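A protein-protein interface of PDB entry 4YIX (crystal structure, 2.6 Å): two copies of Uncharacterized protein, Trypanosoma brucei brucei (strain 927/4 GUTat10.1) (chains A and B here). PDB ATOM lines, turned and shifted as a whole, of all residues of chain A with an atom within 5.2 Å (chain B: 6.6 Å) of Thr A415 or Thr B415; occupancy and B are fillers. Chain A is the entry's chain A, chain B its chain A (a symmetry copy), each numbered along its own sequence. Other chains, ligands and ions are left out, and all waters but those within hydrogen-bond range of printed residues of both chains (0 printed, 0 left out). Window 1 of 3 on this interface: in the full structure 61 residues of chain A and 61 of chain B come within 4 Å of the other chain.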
ATOM      1  N   GLU A 410     -11.841 -25.511   3.045  1.00  0.00           N
ATOM      2  CA  GLU A 410     -12.915 -25.315   2.067  1.00  0.00           C
ATOM      3  C   GLU A 410     -13.888 -26.496   1.995  1.00  0.00           C
ATOM      4  O   GLU A 410     -15.100 -26.305   1.949  1.00  0.00           O
ATOM      5  CB  GLU A 410     -12.309 -25.050   0.680  1.00  0.00           C
ATOM      6  CG  GLU A 410     -13.271 -24.492  -0.360  1.00  0.00           C
ATOM      7  CD  GLU A 410     -12.996 -23.030  -0.718  1.00  0.00           C
ATOM      8  OE1 GLU A 410     -12.855 -22.720  -1.922  1.00  0.00           O
ATOM      9  OE2 GLU A 410     -12.938 -22.177   0.196  1.00  0.00           O
ATOM     10  N   ASP A 411     -13.355 -27.714   2.011  1.00  0.00           N
ATOM     11  CA  ASP A 411     -14.170 -28.907   1.851  1.00  0.00           C
ATOM     12  C   ASP A 411     -15.191 -29.118   2.965  1.00  0.00           C
ATOM     13  O   ASP A 411     -16.249 -29.683   2.712  1.00  0.00           O
ATOM     14  CB  ASP A 411     -13.275 -30.146   1.744  1.00  0.00           C
ATOM     15  CG  ASP A 411     -12.585 -30.256   0.398  1.00  0.00           C
ATOM     16  OD1 ASP A 411     -13.035 -29.590  -0.558  1.00  0.00           O
ATOM     17  OD2 ASP A 411     -11.598 -31.011   0.291  1.00  0.00           O
ATOM     18  N   CYS A 413     -16.343 -26.483   4.761  1.00  0.00           N
ATOM     19  CA  CYS A 413     -17.001 -25.201   4.944  1.00  0.00           C
ATOM     20  C   CYS A 413     -18.356 -25.158   4.265  1.00  0.00           C
ATOM     21  O   CYS A 413     -18.563 -25.782   3.225  1.00  0.00           O
ATOM     22  CB  CYS A 413     -16.138 -24.069   4.400  1.00  0.00           C
ATOM     23  SG  CYS A 413     -15.184 -23.212   5.656  1.00  0.00           S
ATOM     24  N   ALA A 414     -19.278 -24.424   4.873  1.00  0.00           N
ATOM     25  CA  ALA A 414     -20.478 -23.989   4.183  1.00  0.00           C
ATOM     26  C   ALA A 414     -20.052 -22.894   3.227  1.00  0.00           C
ATOM     27  O   ALA A 414     -19.946 -21.740   3.629  1.00  0.00           O
ATOM     28  CB  ALA A 414     -21.515 -23.480   5.162  1.00  0.00           C
ATOM     29  N   THR A 415     -19.831 -23.262   1.992  1.00  0.00           N
ATOM     30  CA  THR A 415     -19.220 -22.383   1.035  1.00  0.00           C
ATOM     31  C   THR A 415     -20.005 -21.137   0.736  1.00  0.00           C
ATOM     32  O   THR A 415     -19.424 -20.158   0.430  1.00  0.00           O
ATOM     33  CB  THR A 415     -18.697 -23.075  -0.233  1.00  0.00           C
ATOM     34  OG1 THR A 415     -19.585 -24.100  -0.639  1.00  0.00           O
ATOM     35  CG2 THR A 415     -17.299 -23.649   0.007  1.00  0.00           C
ATOM     36  N   ASN A 416     -21.309 -21.180   0.829  1.00  0.00           N
ATOM     37  CA  ASN A 416     -22.101 -19.982   0.682  1.00  0.00           C
ATOM     38  C   ASN A 416     -21.812 -18.922   1.752  1.00  0.00           C
ATOM     39  O   ASN A 416     -22.094 -17.791   1.559  1.00  0.00           O
ATOM     40  CB  ASN A 416     -23.569 -20.309   0.570  1.00  0.00           C
ATOM     41  CG  ASN A 416     -24.161 -20.775   1.866  1.00  0.00           C
ATOM     42  OD1 ASN A 416     -25.236 -20.362   2.218  1.00  0.00           O
ATOM     43  ND2 ASN A 416     -23.477 -21.603   2.569  1.00  0.00           N
ATOM     44  N   LEU A 417     -21.358 -19.346   2.908  1.00  0.00           N
ATOM     45  CA  LEU A 417     -20.735 -18.535   3.912  1.00  0.00           C
ATOM     46  C   LEU A 417     -19.409 -17.936   3.523  1.00  0.00           C
ATOM     47  O   LEU A 417     -19.063 -16.915   3.962  1.00  0.00           O
ATOM     48  CB  LEU A 417     -20.617 -19.287   5.222  1.00  0.00           C
ATOM     49  CG  LEU A 417     -20.355 -18.459   6.454  1.00  0.00           C
ATOM     50  CD1 LEU A 417     -21.270 -17.298   6.521  1.00  0.00           C
ATOM     51  CD2 LEU A 417     -20.407 -19.227   7.735  1.00  0.00           C
ATOM     52  N   MET A 418     -18.636 -18.660   2.775  1.00  0.00           N
ATOM     53  CA  MET A 418     -17.345 -18.243   2.345  1.00  0.00           C
ATOM     54  C   MET A 418     -17.218 -17.201   1.241  1.00  0.00           C
ATOM     55  O   MET A 418     -16.445 -16.286   1.348  1.00  0.00           O
ATOM     56  CB  MET A 418     -16.485 -19.477   2.130  1.00  0.00           C
ATOM     57  CG  MET A 418     -16.500 -20.370   3.341  1.00  0.00           C
ATOM     58  SD  MET A 418     -15.638 -19.765   4.789  1.00  0.00           S
ATOM     59  CE  MET A 418     -16.934 -19.361   5.904  1.00  0.00           C
ATOM     60  N   TYR A 419     -18.025 -17.363   0.205  1.00  0.00           N
ATOM     61  CA  TYR A 419     -18.121 -16.447  -0.937  1.00  0.00           C
ATOM     62  C   TYR A 419     -19.397 -16.651  -1.744  1.00  0.00           C
ATOM     63  O   TYR A 419     -20.111 -17.630  -1.553  1.00  0.00           O
ATOM     64  CB  TYR A 419     -16.909 -16.603  -1.862  1.00  0.00           C
ATOM     65  CG  TYR A 419     -16.418 -18.029  -2.010  1.00  0.00           C
ATOM     66  CD1 TYR A 419     -17.177 -18.977  -2.678  1.00  0.00           C
ATOM     67  CD2 TYR A 419     -15.188 -18.421  -1.483  1.00  0.00           C
ATOM     68  CE1 TYR A 419     -16.737 -20.275  -2.815  1.00  0.00           C
ATOM     69  CE2 TYR A 419     -14.737 -19.717  -1.615  1.00  0.00           C
ATOM     70  CZ  TYR A 419     -15.517 -20.642  -2.283  1.00  0.00           C
ATOM     71  OH  TYR A 419     -15.083 -21.941  -2.426  1.00  0.00           O
ATOM     72  N   GLY A 459     -11.852 -23.555  -4.717  1.00  0.00           N
ATOM     73  CA  GLY A 459     -12.632 -23.019  -5.786  1.00  0.00           C
ATOM     74  C   GLY A 459     -12.445 -21.561  -6.065  1.00  0.00           C
ATOM     75  O   GLY A 459     -12.383 -21.176  -7.187  1.00  0.00           O
ATOM     76  N   ALA B 353     -18.086 -35.224  -0.284  1.00  0.00           N
ATOM     77  CA  ALA B 353     -16.718 -35.620  -0.010  1.00  0.00           C
ATOM     78  C   ALA B 353     -16.582 -36.539   1.196  1.00  0.00           C
ATOM     79  O   ALA B 353     -17.358 -36.481   2.091  1.00  0.00           O
ATOM     80  CB  ALA B 353     -15.846 -34.429   0.139  1.00  0.00           C
ATOM     81  N   GLN B 391     -14.473 -38.111  -3.214  1.00  0.00           N
ATOM     82  CA  GLN B 391     -15.767 -37.811  -3.798  1.00  0.00           C
ATOM     83  C   GLN B 391     -15.837 -38.382  -5.197  1.00  0.00           C
ATOM     84  O   GLN B 391     -16.865 -38.928  -5.601  1.00  0.00           O
ATOM     85  CB  GLN B 391     -16.026 -36.309  -3.825  1.00  0.00           C
ATOM     86  CG  GLN B 391     -17.414 -35.962  -4.273  1.00  0.00           C
ATOM     87  CD  GLN B 391     -17.738 -34.504  -4.073  1.00  0.00           C
ATOM     88  OE1 GLN B 391     -16.895 -33.722  -3.649  1.00  0.00           O
ATOM     89  NE2 GLN B 391     -18.970 -34.126  -4.379  1.00  0.00           N
ATOM     90  N   GLU B 410     -23.667 -28.618  -1.804  1.00  0.00           N
ATOM     91  CA  GLU B 410     -22.451 -27.799  -1.821  1.00  0.00           C
ATOM     92  C   GLU B 410     -21.654 -27.875  -0.515  1.00  0.00           C
ATOM     93  O   GLU B 410     -20.433 -27.998  -0.536  1.00  0.00           O
ATOM     94  CB  GLU B 410     -22.817 -26.338  -2.128  1.00  0.00           C
ATOM     95  CG  GLU B 410     -21.651 -25.439  -2.518  1.00  0.00           C
ATOM     96  CD  GLU B 410     -21.666 -25.033  -3.993  1.00  0.00           C
ATOM     97  OE1 GLU B 410     -21.594 -23.819  -4.285  1.00  0.00           O
ATOM     98  OE2 GLU B 410     -21.729 -25.922  -4.871  1.00  0.00           O
ATOM     99  N   ASP B 411     -22.350 -27.826   0.616  1.00  0.00           N
ATOM    100  CA  ASP B 411     -21.697 -27.794   1.914  1.00  0.00           C
ATOM    101  C   ASP B 411     -20.880 -29.042   2.233  1.00  0.00           C
ATOM    102  O   ASP B 411     -19.887 -28.946   2.945  1.00  0.00           O
ATOM    103  CB  ASP B 411     -22.735 -27.573   3.021  1.00  0.00           C
ATOM    104  CG  ASP B 411     -23.240 -26.144   3.072  1.00  0.00           C
ATOM    105  OD1 ASP B 411     -22.574 -25.255   2.503  1.00  0.00           O
ATOM    106  OD2 ASP B 411     -24.299 -25.906   3.687  1.00  0.00           O
ATOM    107  N   THR B 412     -21.292 -30.208   1.737  1.00  0.00           N
ATOM    108  CA  THR B 412     -20.515 -31.437   1.950  1.00  0.00           C
ATOM    109  C   THR B 412     -19.717 -31.850   0.709  1.00  0.00           C
ATOM    110  O   THR B 412     -19.189 -32.957   0.631  1.00  0.00           O
ATOM    111  CB  THR B 412     -21.409 -32.623   2.366  1.00  0.00           C
ATOM    112  OG1 THR B 412     -22.426 -32.822   1.378  1.00  0.00           O
ATOM    113  CG2 THR B 412     -22.052 -32.373   3.723  1.00  0.00           C
ATOM    114  N   CYS B 413     -19.628 -30.959  -0.268  1.00  0.00           N
ATOM    115  CA  CYS B 413     -18.827 -31.221  -1.451  1.00  0.00           C
ATOM    116  C   CYS B 413     -17.400 -30.740  -1.287  1.00  0.00           C
ATOM    117  O   CYS B 413     -17.141 -29.746  -0.612  1.00  0.00           O
ATOM    118  CB  CYS B 413     -19.439 -30.553  -2.676  1.00  0.00           C
ATOM    119  SG  CYS B 413     -20.427 -31.654  -3.692  1.00  0.00           S
ATOM    120  N   ALA B 414     -16.476 -31.466  -1.904  1.00  0.00           N
ATOM    121  CA  ALA B 414     -15.144 -30.948  -2.149  1.00  0.00           C
ATOM    122  C   ALA B 414     -15.274 -29.932  -3.265  1.00  0.00           C
ATOM    123  O   ALA B 414     -15.271 -30.305  -4.434  1.00  0.00           O
ATOM    124  CB  ALA B 414     -14.190 -32.058  -2.538  1.00  0.00           C
ATOM    125  N   THR B 415     -15.372 -28.680  -2.895  1.00  0.00           N
ATOM    126  CA  THR B 415     -15.715 -27.639  -3.823  1.00  0.00           C
ATOM    127  C   THR B 415     -14.728 -27.443  -4.939  1.00  0.00           C
ATOM    128  O   THR B 415     -15.118 -27.050  -5.980  1.00  0.00           O
ATOM    129  CB  THR B 415     -16.150 -26.316  -3.174  1.00  0.00           C
ATOM    130  OG1 THR B 415     -15.368 -26.048  -2.025  1.00  0.00           O
ATOM    131  CG2 THR B 415     -17.635 -26.362  -2.805  1.00  0.00           C
ATOM    132  N   ASN B 416     -13.469 -27.720  -4.719  1.00  0.00           N
ATOM    133  CA  ASN B 416     -12.503 -27.675  -5.792  1.00  0.00           C
ATOM    134  C   ASN B 416     -12.786 -28.684  -6.911  1.00  0.00           C
ATOM    135  O   ASN B 416     -12.323 -28.522  -7.987  1.00  0.00           O
ATOM    136  CB  ASN B 416     -11.095 -27.774  -5.261  1.00  0.00           C
ATOM    137  CG  ASN B 416     -10.760 -29.144  -4.755  1.00  0.00           C
ATOM    138  OD1 ASN B 416      -9.697 -29.640  -5.026  1.00  0.00           O
ATOM    139  ND2 ASN B 416     -11.645 -29.751  -4.050  1.00  0.00           N
ATOM    140  N   LEU B 417     -13.450 -29.768  -6.587  1.00  0.00           N
ATOM    141  CA  LEU B 417     -14.085 -30.667  -7.505  1.00  0.00           C
ATOM    142  C   LEU B 417     -15.248 -30.090  -8.270  1.00  0.00           C
ATOM    143  O   LEU B 417     -15.503 -30.467  -9.341  1.00  0.00           O
ATOM    144  CB  LEU B 417     -14.488 -31.954  -6.814  1.00  0.00           C
ATOM    145  CG  LEU B 417     -14.799 -33.130  -7.705  1.00  0.00           C
ATOM    146  CD1 LEU B 417     -13.748 -33.314  -8.730  1.00  0.00           C
ATOM    147  CD2 LEU B 417     -15.033 -34.412  -6.974  1.00  0.00           C
ATOM    148  N   MET B 418     -16.004 -29.247  -7.639  1.00  0.00           N
ATOM    149  CA  MET B 418     -17.152 -28.636  -8.218  1.00  0.00           C
ATOM    150  C   MET B 418     -16.976 -27.516  -9.236  1.00  0.00           C
ATOM    151  O   MET B 418     -17.620 -27.504 -10.251  1.00  0.00           O
ATOM    152  CB  MET B 418     -18.138 -28.313  -7.108  1.00  0.00           C
ATOM    153  CG  MET B 418     -18.417 -29.521  -6.257  1.00  0.00           C
ATOM    154  SD  MET B 418     -19.376 -30.828  -7.017  1.00  0.00           S
ATOM    155  CE  MET B 418     -18.204 -32.111  -7.270  1.00  0.00           C
ATOM    156  N   TYR B 419     -16.065 -26.605  -8.934  1.00  0.00           N
ATOM    157  CA  TYR B 419     -15.684 -25.480  -9.795  1.00  0.00           C
ATOM    158  C   TYR B 419     -14.350 -24.862  -9.394  1.00  0.00           C
ATOM    159  O   TYR B 419     -13.815 -25.161  -8.331  1.00  0.00           O
ATOM    160  CB  TYR B 419     -16.766 -24.395  -9.782  1.00  0.00           C
ATOM    161  CG  TYR B 419     -17.428 -24.192  -8.434  1.00  0.00           C
ATOM    162  CD1 TYR B 419     -16.725 -23.646  -7.371  1.00  0.00           C
ATOM    163  CD2 TYR B 419     -18.761 -24.544  -8.230  1.00  0.00           C
ATOM    164  CE1 TYR B 419     -17.320 -23.460  -6.144  1.00  0.00           C
ATOM    165  CE2 TYR B 419     -19.369 -24.361  -7.006  1.00  0.00           C
ATOM    166  CZ  TYR B 419     -18.641 -23.818  -5.964  1.00  0.00           C
ATOM    167  OH  TYR B 419     -19.230 -23.626  -4.733  1.00  0.00           O
ATOM    168  N   ARG B 420     -13.821 -24.003 -10.264  1.00  0.00           N
ATOM    169  CA  ARG B 420     -12.648 -23.176  -9.959  1.00  0.00           C
ATOM    170  C   ARG B 420     -12.763 -21.846 -10.691  1.00  0.00           C
ATOM    171  O   ARG B 420     -12.932 -21.826 -11.904  1.00  0.00           O
ATOM    172  CB  ARG B 420     -11.345 -23.881 -10.361  1.00  0.00           C
ATOM    173  CG  ARG B 420     -10.951 -25.065  -9.488  1.00  0.00           C
ATOM    174  CD  ARG B 420      -9.778 -25.807 -10.104  1.00  0.00           C
ATOM    175  NE  ARG B 420      -8.539 -25.022 -10.105  1.00  0.00           N
ATOM    176  CZ  ARG B 420      -7.766 -24.826 -11.174  1.00  0.00           C
ATOM    177  NH1 ARG B 420      -8.105 -25.342 -12.350  1.00  0.00           N
ATOM    178  NH2 ARG B 420      -6.652 -24.113 -11.068  1.00  0.00           N
ATOM    179  N   GLY B 458     -24.558 -23.001  -3.599  1.00  0.00           N
ATOM    180  CA  GLY B 458     -24.525 -21.671  -3.065  1.00  0.00           C
ATOM    181  C   GLY B 458     -23.583 -20.687  -3.682  1.00  0.00           C
ATOM    182  O   GLY B 458     -23.985 -19.749  -4.276  1.00  0.00           O
ATOM    183  N   GLY B 459     -22.309 -20.917  -3.517  1.00  0.00           N
ATOM    184  CA  GLY B 459     -21.321 -19.965  -3.910  1.00  0.00           C
ATOM    185  C   GLY B 459     -21.260 -19.649  -5.371  1.00  0.00           C
ATOM    186  O   GLY B 459     -21.112 -18.526  -5.729  1.00  0.00           O
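Among the printed residues, pairs that only touch across the chains: Ala A414 with Asp B411 (3.0 Å), Asp A411 with Ala B414 (3.0 Å), Glu A410 with Thr B415 (3.1 Å), Thr A415 with Glu B410 (3.1 Å), Gly A459 with Arg B420 (3.4 Å), Gly A459 with Tyr B419 (3.5 Å), Tyr A419 with Gly B459 (3.5 Å), Thr A415 with Thr B415 (3.7 Å), Asp A411 with Asp B411 (3.7 Å), Asp A411 with Asn B416 (3.8 Å), Asn A416 with Asp B411 (3.8 Å) and Asn A416 with Gly B458 (3.998 Å).
Glu A410 touches Thr B415, and with the chains exchanged Thr A415 touches Glu B410. Asp A411 touches Ala B414, and with the chains exchanged Ala A414 touches Asp B411. Asp A411 touches Asn B416, and with the chains exchanged Asn A416 touches Asp B411. Tyr A419 touches Gly B459, and with the chains exchanged Gly A459 touches Tyr B419. Of the 16 pairs that touch across the chains among the printed residues, 14 have their exchanged pair printed and touching as well.
Hydrophobic or aromatic side chains of chain B that line the printed part of chain A: Ala B414. Printed residues of chain A that touch a printed residue of chain B: Glu A410, Asp A411, Cys A413, Ala A414, Thr A415, Asn A416, Tyr A419 and Gly A459. Among the printed residues, 16 pairs touch across the chains.
Of chain B, only Glu B410, Asp B411 and Thr B415 come within 4 Å of Thr A415. Of the printed residues of chain A, Gly B458 touches Asn A416. Of the printed residues of chain B, Asp A411 touches Asp B411, Cys B413, Ala B414, Thr B415 and Asn B416. Of the printed residues of chain B, Tyr A419 touches Gly B459 (3.5 Å). Printed residues of chain A within 4 Å of Arg B420: Gly A459. Met B418 touches none of the printed residues of chain A. The nearest residue of chain B that does not touch Thr A415 is Tyr B419 (4.1 Å).
The backbone NH (N) of Thr B415 lies within hydrogen-bond range of the side-chain carboxylate (OD1) of Asp A411, 3.4 Å away. The backbone NH (N) of Thr A415 lies within hydrogen-bond range of the side-chain carboxylate (OD1) of Asp B411 (3.4 Å). O of Asp A411 sits close to O of Cys B413 (3.4 Å). The backbone carbonyl oxygen (O) of Asp B411 lies close to the backbone carbonyl oxygen (O) of Cys A413, 3.4 Å away.
The side-chain carboxylate of Glu A410 sits at hydrogen-bond distance from the side-chain hydroxyl of Tyr A419, 2.4 Å away. The side-chain carboxylate (OE1) of Glu A410 is in hydrogen-bond range of the backbone NH (N) of Gly A459, at 3.1 Å. NE2 of Gln B391 sits close to SG of Cys B413 (3.0 Å). The side-chain amide oxygen (OE1) of Gln B391 is in hydrogen-bond range of the backbone NH (N) of Ala B414, at 2.9 Å. The side-chain carboxylate of Glu B410 lies within hydrogen-bond range of the backbone NH of Gly B458, 3.2 Å away. The side-chain carboxylate (OE1) of Glu B410 lies within hydrogen-bond range of the backbone NH (N) of Gly B459 (3.1 Å).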
